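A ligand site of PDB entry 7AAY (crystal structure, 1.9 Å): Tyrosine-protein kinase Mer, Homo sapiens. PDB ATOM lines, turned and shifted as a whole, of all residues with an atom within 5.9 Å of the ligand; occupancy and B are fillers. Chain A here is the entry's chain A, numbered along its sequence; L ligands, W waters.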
ATOM      1  N   LEU A  27       4.796  13.483   0.319  1.00  0.00           N
ATOM      2  CA  LEU A  27       4.146  13.344   1.617  1.00  0.00           C
ATOM      3  C   LEU A  27       2.639  13.420   1.482  1.00  0.00           C
ATOM      4  O   LEU A  27       1.924  12.716   2.181  1.00  0.00           O
ATOM      5  CB  LEU A  27       4.628  14.424   2.581  1.00  0.00           C
ATOM      6  CG  LEU A  27       6.129  14.379   2.905  1.00  0.00           C
ATOM      7  CD1 LEU A  27       6.599  15.664   3.565  1.00  0.00           C
ATOM      8  CD2 LEU A  27       6.422  13.169   3.777  1.00  0.00           C
ATOM      9  N   GLY A  28       2.158  14.277   0.591  1.00  0.00           N
ATOM     10  CA  GLY A  28       0.728  14.383   0.294  1.00  0.00           C
ATOM     11  C   GLY A  28       0.439  15.612  -0.524  1.00  0.00           C
ATOM     12  O   GLY A  28       1.374  16.284  -0.989  1.00  0.00           O
ATOM     13  N   GLU A  29      -0.847  15.920  -0.706  1.00  0.00           N
ATOM     14  CA  GLU A  29      -1.262  17.116  -1.439  1.00  0.00           C
ATOM     15  C   GLU A  29      -1.648  18.249  -0.479  1.00  0.00           C
ATOM     16  O   GLU A  29      -2.248  18.000   0.567  1.00  0.00           O
ATOM     17  CB  GLU A  29      -2.454  16.790  -2.364  1.00  0.00           C
ATOM     18  CG  GLU A  29      -2.118  15.822  -3.496  1.00  0.00           C
ATOM     19  CD  GLU A  29      -1.042  16.339  -4.451  1.00  0.00           C
ATOM     20  OE1 GLU A  29      -1.042  17.544  -4.788  1.00  0.00           O
ATOM     21  OE2 GLU A  29      -0.175  15.534  -4.866  1.00  0.00           O
ATOM     22  N   GLY A  30      -1.290  19.475  -0.848  1.00  0.00           N
ATOM     23  CA  GLY A  30      -1.670  20.689  -0.129  1.00  0.00           C
ATOM     24  C   GLY A  30      -2.503  21.614  -0.996  1.00  0.00           C
ATOM     25  O   GLY A  30      -2.952  21.214  -2.070  1.00  0.00           O
ATOM     26  N   VAL A  35       3.156  18.047  -1.590  1.00  0.00           N
ATOM     27  CA  VAL A  35       4.103  18.371  -0.524  1.00  0.00           C
ATOM     28  C   VAL A  35       5.121  17.237  -0.510  1.00  0.00           C
ATOM     29  O   VAL A  35       4.743  16.088  -0.295  1.00  0.00           O
ATOM     30  CB  VAL A  35       3.398  18.531   0.852  1.00  0.00           C
ATOM     31  CG1 VAL A  35       4.429  18.756   1.958  1.00  0.00           C
ATOM     32  CG2 VAL A  35       2.402  19.681   0.791  1.00  0.00           C
ATOM     33  N   ALA A  51      10.044  19.540   4.830  1.00  0.00           N
ATOM     34  CA  ALA A  51       8.878  19.355   3.973  1.00  0.00           C
ATOM     35  C   ALA A  51       8.877  20.534   3.011  1.00  0.00           C
ATOM     36  O   ALA A  51       9.149  21.674   3.405  1.00  0.00           O
ATOM     37  CB  ALA A  51       7.605  19.334   4.787  1.00  0.00           C
ATOM     38  N   VAL A  52       8.583  20.247   1.753  1.00  0.00           N
ATOM     39  CA  VAL A  52       8.652  21.256   0.689  1.00  0.00           C
ATOM     40  C   VAL A  52       7.313  21.383   0.013  1.00  0.00           C
ATOM     41  O   VAL A  52       6.822  20.452  -0.625  1.00  0.00           O
ATOM     42  CB  VAL A  52       9.742  20.972  -0.356  1.00  0.00           C
ATOM     43  CG1 VAL A  52       9.918  22.169  -1.277  1.00  0.00           C
ATOM     44  CG2 VAL A  52      11.054  20.656   0.344  1.00  0.00           C
ATOM     45  N   LYS A  53       6.737  22.573   0.163  1.00  0.00           N
ATOM     46  CA  LYS A  53       5.428  22.901  -0.372  1.00  0.00           C
ATOM     47  C   LYS A  53       5.682  23.423  -1.784  1.00  0.00           C
ATOM     48  O   LYS A  53       6.455  24.380  -1.957  1.00  0.00           O
ATOM     49  CB  LYS A  53       4.798  23.967   0.525  1.00  0.00           C
ATOM     50  CG  LYS A  53       3.315  24.236   0.356  1.00  0.00           C
ATOM     51  CD  LYS A  53       2.983  25.512   1.122  1.00  0.00           C
ATOM     52  CE  LYS A  53       1.504  25.789   1.268  1.00  0.00           C
ATOM     53  NZ  LYS A  53       1.325  27.144   1.880  1.00  0.00           N
ATOM     54  N   GLU A  71       1.192  33.647   1.971  1.00  0.00           N
ATOM     55  CA  GLU A  71       1.182  32.700   3.091  1.00  0.00           C
ATOM     56  C   GLU A  71       2.550  32.540   3.742  1.00  0.00           C
ATOM     57  O   GLU A  71       2.657  32.511   4.962  1.00  0.00           O
ATOM     58  CB  GLU A  71       0.628  31.342   2.633  1.00  0.00           C
ATOM     59  CG  GLU A  71      -0.873  31.360   2.412  1.00  0.00           C
ATOM     60  CD  GLU A  71      -1.404  30.101   1.762  1.00  0.00           C
ATOM     61  OE1 GLU A  71      -0.732  29.047   1.827  1.00  0.00           O
ATOM     62  OE2 GLU A  71      -2.510  30.157   1.170  1.00  0.00           O
ATOM     63  N   ALA A  72       3.598  32.450   2.929  1.00  0.00           N
ATOM     64  CA  ALA A  72       4.965  32.352   3.401  1.00  0.00           C
ATOM     65  C   ALA A  72       5.373  33.629   4.101  1.00  0.00           C
ATOM     66  O   ALA A  72       5.936  33.581   5.192  1.00  0.00           O
ATOM     67  CB  ALA A  72       5.936  32.079   2.240  1.00  0.00           C
ATOM     68  N   CYS A  74       3.366  35.718   5.457  1.00  0.00           N
ATOM     69  CA  CYS A  74       2.600  35.732   6.704  1.00  0.00           C
ATOM     70  C   CYS A  74       3.269  34.958   7.848  1.00  0.00           C
ATOM     71  O   CYS A  74       3.288  35.424   8.982  1.00  0.00           O
ATOM     72  CB  CYS A  74       1.195  35.190   6.454  1.00  0.00           C
ATOM     73  SG  CYS A  74       0.168  35.392   7.901  1.00  0.00           S
ATOM     74  N   MET A  75       3.826  33.784   7.538  1.00  0.00           N
ATOM     75  CA  MET A  75       4.591  32.965   8.489  1.00  0.00           C
ATOM     76  C   MET A  75       5.952  33.480   8.904  1.00  0.00           C
ATOM     77  O   MET A  75       6.511  32.995   9.896  1.00  0.00           O
ATOM     78  CB  MET A  75       4.928  31.615   7.861  1.00  0.00           C
ATOM     79  CG  MET A  75       3.829  30.605   7.900  1.00  0.00           C
ATOM     80  SD  MET A  75       4.420  29.024   7.297  1.00  0.00           S
ATOM     81  CE  MET A  75       5.594  28.570   8.557  1.00  0.00           C
ATOM     82  N   PHE A  78       7.184  34.268  12.536  1.00  0.00           N
ATOM     83  CA  PHE A  78       6.769  33.332  13.602  1.00  0.00           C
ATOM     84  C   PHE A  78       7.978  32.579  14.100  1.00  0.00           C
ATOM     85  O   PHE A  78       8.575  31.783  13.364  1.00  0.00           O
ATOM     86  CB  PHE A  78       5.726  32.290  13.135  1.00  0.00           C
ATOM     87  CG  PHE A  78       4.409  32.860  12.705  1.00  0.00           C
ATOM     88  CD1 PHE A  78       4.048  34.189  12.962  1.00  0.00           C
ATOM     89  CD2 PHE A  78       3.502  32.040  12.052  1.00  0.00           C
ATOM     90  CE1 PHE A  78       2.819  34.670  12.542  1.00  0.00           C
ATOM     91  CE2 PHE A  78       2.266  32.516  11.654  1.00  0.00           C
ATOM     92  CZ  PHE A  78       1.923  33.835  11.901  1.00  0.00           C
ATOM     93  N   VAL A  83       4.751  26.695  17.203  1.00  0.00           N
ATOM     94  CA  VAL A  83       4.235  27.258  15.967  1.00  0.00           C
ATOM     95  C   VAL A  83       5.166  26.802  14.850  1.00  0.00           C
ATOM     96  O   VAL A  83       6.402  26.869  14.982  1.00  0.00           O
ATOM     97  CB  VAL A  83       4.171  28.794  16.036  1.00  0.00           C
ATOM     98  CG1 VAL A  83       3.545  29.383  14.769  1.00  0.00           C
ATOM     99  CG2 VAL A  83       3.385  29.254  17.268  1.00  0.00           C
ATOM    100  N   ILE A  84       4.579  26.301  13.776  1.00  0.00           N
ATOM    101  CA  ILE A  84       5.376  25.944  12.577  1.00  0.00           C
ATOM    102  C   ILE A  84       6.214  27.152  12.095  1.00  0.00           C
ATOM    103  O   ILE A  84       5.759  28.287  12.167  1.00  0.00           O
ATOM    104  CB  ILE A  84       4.470  25.389  11.459  1.00  0.00           C
ATOM    105  CG1 ILE A  84       5.316  24.742  10.362  1.00  0.00           C
ATOM    106  CG2 ILE A  84       3.563  26.469  10.874  1.00  0.00           C
ATOM    107  CD1 ILE A  84       4.521  23.878   9.408  1.00  0.00           C
ATOM    108  N   VAL A  99       8.072  26.588  -0.840  1.00  0.00           N
ATOM    109  CA  VAL A  99       8.195  27.003   0.559  1.00  0.00           C
ATOM    110  C   VAL A  99       8.760  25.814   1.325  1.00  0.00           C
ATOM    111  O   VAL A  99       8.224  24.702   1.230  1.00  0.00           O
ATOM    112  CB  VAL A  99       6.810  27.425   1.145  1.00  0.00           C
ATOM    113  CG1 VAL A  99       6.894  27.718   2.639  1.00  0.00           C
ATOM    114  CG2 VAL A  99       6.257  28.635   0.397  1.00  0.00           C
ATOM    115  N   LEU A 101       9.564  24.006   4.872  1.00  0.00           N
ATOM    116  CA  LEU A 101       9.109  23.902   6.260  1.00  0.00           C
ATOM    117  C   LEU A 101       9.794  22.719   6.976  1.00  0.00           C
ATOM    118  O   LEU A 101      10.290  21.807   6.313  1.00  0.00           O
ATOM    119  CB  LEU A 101       7.593  23.693   6.272  1.00  0.00           C
ATOM    120  CG  LEU A 101       6.707  24.635   5.454  1.00  0.00           C
ATOM    121  CD1 LEU A 101       5.313  24.025   5.318  1.00  0.00           C
ATOM    122  CD2 LEU A 101       6.655  26.012   6.079  1.00  0.00           C
ATOM    123  N   PRO A 102       9.779  22.694   8.332  1.00  0.00           N
ATOM    124  CA  PRO A 102      10.386  21.584   9.051  1.00  0.00           C
ATOM    125  C   PRO A 102       9.577  20.320   8.920  1.00  0.00           C
ATOM    126  O   PRO A 102       8.352  20.373   8.795  1.00  0.00           O
ATOM    127  CB  PRO A 102      10.399  22.056  10.514  1.00  0.00           C
ATOM    128  CG  PRO A 102       9.947  23.470  10.484  1.00  0.00           C
ATOM    129  CD  PRO A 102       9.107  23.598   9.259  1.00  0.00           C
ATOM    130  N   PHE A 103      10.260  19.183   8.920  1.00  0.00           N
ATOM    131  CA  PHE A 103       9.620  17.894   8.847  1.00  0.00           C
ATOM    132  C   PHE A 103       8.987  17.595  10.203  1.00  0.00           C
ATOM    133  O   PHE A 103       9.615  17.826  11.241  1.00  0.00           O
ATOM    134  CB  PHE A 103      10.645  16.823   8.449  1.00  0.00           C
ATOM    135  CG  PHE A 103      10.040  15.505   8.109  1.00  0.00           C
ATOM    136  CD1 PHE A 103       9.364  15.339   6.909  1.00  0.00           C
ATOM    137  CD2 PHE A 103      10.095  14.425   9.005  1.00  0.00           C
ATOM    138  CE1 PHE A 103       8.769  14.125   6.579  1.00  0.00           C
ATOM    139  CE2 PHE A 103       9.503  13.206   8.684  1.00  0.00           C
ATOM    140  CZ  PHE A 103       8.843  13.050   7.461  1.00  0.00           C
ATOM    141  N   MET A 104       7.742  17.121  10.185  1.00  0.00           N
ATOM    142  CA  MET A 104       6.995  16.805  11.410  1.00  0.00           C
ATOM    143  C   MET A 104       6.807  15.313  11.424  1.00  0.00           C
ATOM    144  O   MET A 104       5.911  14.790  10.768  1.00  0.00           O
ATOM    145  CB  MET A 104       5.646  17.516  11.403  1.00  0.00           C
ATOM    146  CG  MET A 104       5.737  19.031  11.352  1.00  0.00           C
ATOM    147  SD  MET A 104       6.528  19.662  12.821  1.00  0.00           S
ATOM    148  CE  MET A 104       6.886  21.347  12.332  1.00  0.00           C
ATOM    149  N   LYS A 105       7.650  14.636  12.184  1.00  0.00           N
ATOM    150  CA  LYS A 105       7.813  13.182  12.051  1.00  0.00           C
ATOM    151  C   LYS A 105       6.497  12.426  12.144  1.00  0.00           C
ATOM    152  O   LYS A 105       6.223  11.562  11.326  1.00  0.00           O
ATOM    153  CB  LYS A 105       8.809  12.649  13.081  1.00  0.00           C
ATOM    154  CG  LYS A 105       9.078  11.137  12.965  1.00  0.00           C
ATOM    155  CD  LYS A 105      10.259  10.704  13.817  1.00  0.00           C
ATOM    156  CE  LYS A 105      10.420   9.196  13.866  1.00  0.00           C
ATOM    157  NZ  LYS A 105      11.800   8.837  14.328  1.00  0.00           N
ATOM    158  N   GLY A 107       3.347  13.596  11.853  1.00  0.00           N
ATOM    159  CA  GLY A 107       2.239  14.106  11.047  1.00  0.00           C
ATOM    160  C   GLY A 107       1.210  14.876  11.882  1.00  0.00           C
ATOM    161  O   GLY A 107       1.526  15.404  12.968  1.00  0.00           O
ATOM    162  N   MET A 141      -0.819  29.285  20.555  1.00  0.00           N
ATOM    163  CA  MET A 141      -1.899  30.268  20.376  1.00  0.00           C
ATOM    164  C   MET A 141      -1.711  31.538  21.205  1.00  0.00           C
ATOM    165  O   MET A 141      -1.996  32.618  20.720  1.00  0.00           O
ATOM    166  CB  MET A 141      -3.267  29.620  20.641  1.00  0.00           C
ATOM    167  CG  MET A 141      -3.650  28.541  19.597  1.00  0.00           C
ATOM    168  SD  MET A 141      -3.539  29.093  17.878  1.00  0.00           S
ATOM    169  CE  MET A 141      -4.667  30.490  17.850  1.00  0.00           C
ATOM    170  N   LEU A 144       0.656  33.553  19.161  1.00  0.00           N
ATOM    171  CA  LEU A 144       0.057  34.082  17.948  1.00  0.00           C
ATOM    172  C   LEU A 144      -0.946  35.203  18.246  1.00  0.00           C
ATOM    173  O   LEU A 144      -0.923  36.253  17.562  1.00  0.00           O
ATOM    174  CB  LEU A 144      -0.590  32.962  17.126  1.00  0.00           C
ATOM    175  CG  LEU A 144       0.410  31.952  16.534  1.00  0.00           C
ATOM    176  CD1 LEU A 144      -0.322  30.732  16.017  1.00  0.00           C
ATOM    177  CD2 LEU A 144       1.269  32.585  15.442  1.00  0.00           C
ATOM    178  N   PHE A 149      -2.394  37.579  15.321  1.00  0.00           N
ATOM    179  CA  PHE A 149      -2.654  36.642  14.244  1.00  0.00           C
ATOM    180  C   PHE A 149      -3.925  35.859  14.598  1.00  0.00           C
ATOM    181  O   PHE A 149      -4.038  35.361  15.708  1.00  0.00           O
ATOM    182  CB  PHE A 149      -1.468  35.697  14.071  1.00  0.00           C
ATOM    183  CG  PHE A 149      -1.687  34.636  13.037  1.00  0.00           C
ATOM    184  CD1 PHE A 149      -1.452  34.899  11.684  1.00  0.00           C
ATOM    185  CD2 PHE A 149      -2.138  33.371  13.408  1.00  0.00           C
ATOM    186  CE1 PHE A 149      -1.653  33.915  10.727  1.00  0.00           C
ATOM    187  CE2 PHE A 149      -2.357  32.377  12.452  1.00  0.00           C
ATOM    188  CZ  PHE A 149      -2.111  32.645  11.120  1.00  0.00           C
ATOM    189  N   HIS A 151      -6.044  32.513  13.696  1.00  0.00           N
ATOM    190  CA  HIS A 151      -5.929  31.222  13.032  1.00  0.00           C
ATOM    191  C   HIS A 151      -7.106  30.965  12.076  1.00  0.00           C
ATOM    192  O   HIS A 151      -6.887  30.782  10.889  1.00  0.00           O
ATOM    193  CB  HIS A 151      -5.784  30.081  14.055  1.00  0.00           C
ATOM    194  CG  HIS A 151      -5.228  28.821  13.475  1.00  0.00           C
ATOM    195  ND1 HIS A 151      -5.883  28.091  12.513  1.00  0.00           N
ATOM    196  CD2 HIS A 151      -4.064  28.173  13.713  1.00  0.00           C
ATOM    197  CE1 HIS A 151      -5.150  27.048  12.170  1.00  0.00           C
ATOM    198  NE2 HIS A 151      -4.036  27.071  12.889  1.00  0.00           N
ATOM    199  N   MET A 160       0.494  19.653  14.390  1.00  0.00           N
ATOM    200  CA  MET A 160       1.463  18.726  13.906  1.00  0.00           C
ATOM    201  C   MET A 160       2.370  18.296  15.025  1.00  0.00           C
ATOM    202  O   MET A 160       2.694  19.082  15.905  1.00  0.00           O
ATOM    203  CB  MET A 160       2.249  19.360  12.769  1.00  0.00           C
ATOM    204  CG  MET A 160       1.339  19.917  11.675  1.00  0.00           C
ATOM    205  SD  MET A 160       2.211  20.166  10.133  1.00  0.00           S
ATOM    206  CE  MET A 160       2.389  18.464   9.590  1.00  0.00           C
ATOM    207  N   VAL A 169       1.412  24.330  16.088  1.00  0.00           N
ATOM    208  CA  VAL A 169       0.219  24.843  15.428  1.00  0.00           C
ATOM    209  C   VAL A 169       0.594  25.235  13.994  1.00  0.00           C
ATOM    210  O   VAL A 169       1.672  25.785  13.736  1.00  0.00           O
ATOM    211  CB  VAL A 169      -0.389  26.018  16.217  1.00  0.00           C
ATOM    212  CG1 VAL A 169      -1.588  26.593  15.496  1.00  0.00           C
ATOM    213  CG2 VAL A 169      -0.812  25.544  17.594  1.00  0.00           C
ATOM    214  N   ALA A 170      -0.314  24.920  13.070  1.00  0.00           N
ATOM    215  CA  ALA A 170      -0.121  25.189  11.652  1.00  0.00           C
ATOM    216  C   ALA A 170      -1.478  25.228  10.976  1.00  0.00           C
ATOM    217  O   ALA A 170      -2.522  25.176  11.629  1.00  0.00           O
ATOM    218  CB  ALA A 170       0.761  24.101  11.041  1.00  0.00           C
ATOM    219  N   ASP A 171      -1.465  25.359   9.659  1.00  0.00           N
ATOM    220  CA  ASP A 171      -2.661  25.268   8.833  1.00  0.00           C
ATOM    221  C   ASP A 171      -2.332  24.588   7.515  1.00  0.00           C
ATOM    222  O   ASP A 171      -1.494  25.077   6.766  1.00  0.00           O
ATOM    223  CB  ASP A 171      -3.226  26.672   8.583  1.00  0.00           C
ATOM    224  CG  ASP A 171      -4.658  26.644   8.109  1.00  0.00           C
ATOM    225  OD1 ASP A 171      -5.109  25.598   7.600  1.00  0.00           O
ATOM    226  OD2 ASP A 171      -5.341  27.678   8.246  1.00  0.00           O
ATOM    227  N   PHE A 172      -2.990  23.467   7.250  1.00  0.00           N
ATOM    228  CA  PHE A 172      -2.786  22.692   6.011  1.00  0.00           C
ATOM    229  C   PHE A 172      -3.364  23.360   4.764  1.00  0.00           C
ATOM    230  O   PHE A 172      -2.823  23.173   3.673  1.00  0.00           O
ATOM    231  CB  PHE A 172      -3.329  21.261   6.138  1.00  0.00           C
ATOM    232  CG  PHE A 172      -2.425  20.346   6.929  1.00  0.00           C
ATOM    233  CD1 PHE A 172      -2.424  20.375   8.316  1.00  0.00           C
ATOM    234  CD2 PHE A 172      -1.576  19.469   6.289  1.00  0.00           C
ATOM    235  CE1 PHE A 172      -1.607  19.543   9.048  1.00  0.00           C
ATOM    236  CE2 PHE A 172      -0.753  18.625   7.025  1.00  0.00           C
ATOM    237  CZ  PHE A 172      -0.767  18.661   8.408  1.00  0.00           C
HETATM  238  C1  LIG L   1      -1.259  29.052  10.032  1.00  0.00           C
HETATM  239  C2  LIG L   1       1.051  28.951  10.679  1.00  0.00           C
HETATM  240  C3  LIG L   1       1.326  22.982   6.807  1.00  0.00           C
HETATM  241  C4  LIG L   1       1.429  21.662   6.421  1.00  0.00           C
HETATM  242  C5  LIG L   1      -1.634  29.045  11.379  1.00  0.00           C
HETATM  243  C6  LIG L   1       0.693  28.933  12.016  1.00  0.00           C
HETATM  244  C7  LIG L   1       3.854  19.605   6.093  1.00  0.00           C
HETATM  245  C8  LIG L   1       3.280  16.849   5.867  1.00  0.00           C
HETATM  246  C9  LIG L   1       2.024  23.692   4.615  1.00  0.00           C
HETATM  247  C10 LIG L   1       5.794  18.706   7.590  1.00  0.00           C
HETATM  248  C11 LIG L   1       0.631  18.015   3.385  1.00  0.00           C
HETATM  249  C12 LIG L   1       0.701  16.101   4.464  1.00  0.00           C
HETATM  250  C13 LIG L   1       4.656  18.671   6.748  1.00  0.00           C
HETATM  251  C14 LIG L   1       2.479  17.799   5.208  1.00  0.00           C
HETATM  252  C15 LIG L   1       1.329  17.335   4.389  1.00  0.00           C
HETATM  253  C16 LIG L   1       4.354  17.298   6.625  1.00  0.00           C
HETATM  254  C17 LIG L   1       0.087  29.001   9.690  1.00  0.00           C
HETATM  255  C18 LIG L   1       1.612  23.998   5.914  1.00  0.00           C
HETATM  256  C19 LIG L   1       1.835  21.346   5.131  1.00  0.00           C
HETATM  257  C20 LIG L   1       2.780  19.156   5.335  1.00  0.00           C
HETATM  258  C21 LIG L   1      -0.644  28.986  12.321  1.00  0.00           C
HETATM  259  C22 LIG L   1       2.116  22.373   4.257  1.00  0.00           C
HETATM  260  C23 LIG L   1       1.248  28.925   5.670  1.00  0.00           C
HETATM  261  C24 LIG L   1       0.919  30.157   6.265  1.00  0.00           C
HETATM  262  C25 LIG L   1       1.207  27.749   6.371  1.00  0.00           C
HETATM  263  C26 LIG L   1       0.532  30.207   7.574  1.00  0.00           C
HETATM  264  C27 LIG L   1       0.802  27.740   7.774  1.00  0.00           C
HETATM  265  C28 LIG L   1       1.580  26.505   5.629  1.00  0.00           C
HETATM  266  C29 LIG L   1       0.169  31.486   8.248  1.00  0.00           C
HETATM  267  C30 LIG L   1       5.420  15.197   7.557  1.00  0.00           C
HETATM  268  N1  LIG L   1       6.170  17.495   7.948  1.00  0.00           N
HETATM  269  N2  LIG L   1      -0.336  17.274   2.882  1.00  0.00           N
HETATM  270  N3  LIG L   1      -0.279  16.106   3.552  1.00  0.00           N
HETATM  271  N4  LIG L   1       5.291  16.635   7.360  1.00  0.00           N
HETATM  272  N5  LIG L   1       0.478  29.016   8.306  1.00  0.00           N
HETATM  273  N6  LIG L   1       1.488  25.339   6.351  1.00  0.00           N
HETATM  274  O1  LIG L   1       0.739  26.739   8.471  1.00  0.00           O
HETATM  275  O2  LIG L   1       1.940  26.576   4.455  1.00  0.00           O
HETATM  276  O3  LIG L   1       1.965  20.051   4.668  1.00  0.00           O
HETATM  277  F1  LIG L   1      -0.998  28.978  13.626  1.00  0.00           F
HETATM  278  F2  LIG L   1       2.510  22.063   3.009  1.00  0.00           F
HETATM  279  O   HOH W   1      -4.558  29.748   9.778  1.00  0.00           O
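The side-chain amino group (NZ) of Lys 53 sits at hydrogen-bond distance from an oxygen (O2) of the ligand.
The backbone NH of Met 104 sits at hydrogen-bond distance from a nitrogen (N1) of the ligand (2.8 Å).
N of Asp 171 lies within hydrogen-bond range of O1 of the ligand, 2.9 Å away.
O of Asp 171 sits at hydrogen-bond distance from N6 of the ligand (3.0 Å).
The backbone carbonyl oxygen (O) of Glu 29 sits at hydrogen-bond distance from a nitrogen (N2) of the ligand.
OE1 of Glu 71 lies within salt-bridge range of NZ of Lys 53.
The backbone NH of Lys 53 lies within hydrogen-bond range of the backbone carbonyl oxygen of Val 99.
The backbone carbonyl oxygen of Leu 144 sits at hydrogen-bond distance from the backbone NH of Phe 149 (3.0 Å).
The backbone NH (N) of Ile 84 lies within hydrogen-bond range of the backbone carbonyl oxygen (O) of Val 169, at 3.0 Å.
A ring nitrogen (NE2) of His 151 lies within hydrogen-bond range of the backbone carbonyl oxygen (O) of Ala 170.
N of Val 35 sits at hydrogen-bond distance from O of Gly 28 (2.6 Å).
O of Val 35 is in hydrogen-bond range of N of Leu 27, at 2.7 Å.
The backbone NH of Ala 51 is in hydrogen-bond range of the backbone carbonyl oxygen of Leu 101.
Gly 28 touches the ligand.
Val 35 touches the ligand.
Ala 51 touches the ligand.
O of Glu 71 touches C24 of the ligand, 3.2 Å away.
SG of Cys 74 touches C29 of the ligand, 3.9 Å away.
CG of Met 75 touches C26 of the ligand, 3.3 Å away.
Phe 78 touches the ligand.
CG1 of Val 83 touches C6 of the ligand, at 3.99 Å.
Ile 84 touches the ligand.
Leu 101 touches the ligand (CD1 to C9, 3.4 Å).
Pro 102 touches the ligand (O to C10, 3.3 Å).
CA of Phe 103 touches N1 of the ligand, at 3.6 Å.
Leu 144 touches the ligand (CD1 to F1, 3.0 Å).
Phe 149 touches the ligand.
CD2 of His 151 touches F1 of the ligand, at 3.2 Å.
Met 160 touches the ligand.
CG1 of Val 169 touches F1 of the ligand (3.1 Å).
Ala 170 touches the ligand (CA to O1, 3.6 Å).
Phe 172 touches the ligand.
23 residues have an atom within 4 Å of the ligand: Gly 28, Glu 29, Val 35, Ala 51, Lys 53, Glu 71, Cys 74, Met 75, Phe 78, Val 83, Ile 84, Leu 101, Pro 102, Phe 103, Met 104, Leu 144, Phe 149, His 151, Met 160, Val 169, Ala 170, Asp 171 and Phe 172.
Water W1 lies within hydrogen-bond range of OD2 of Asp 171 (2.7 Å) and O of His 151 (2.8 Å).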
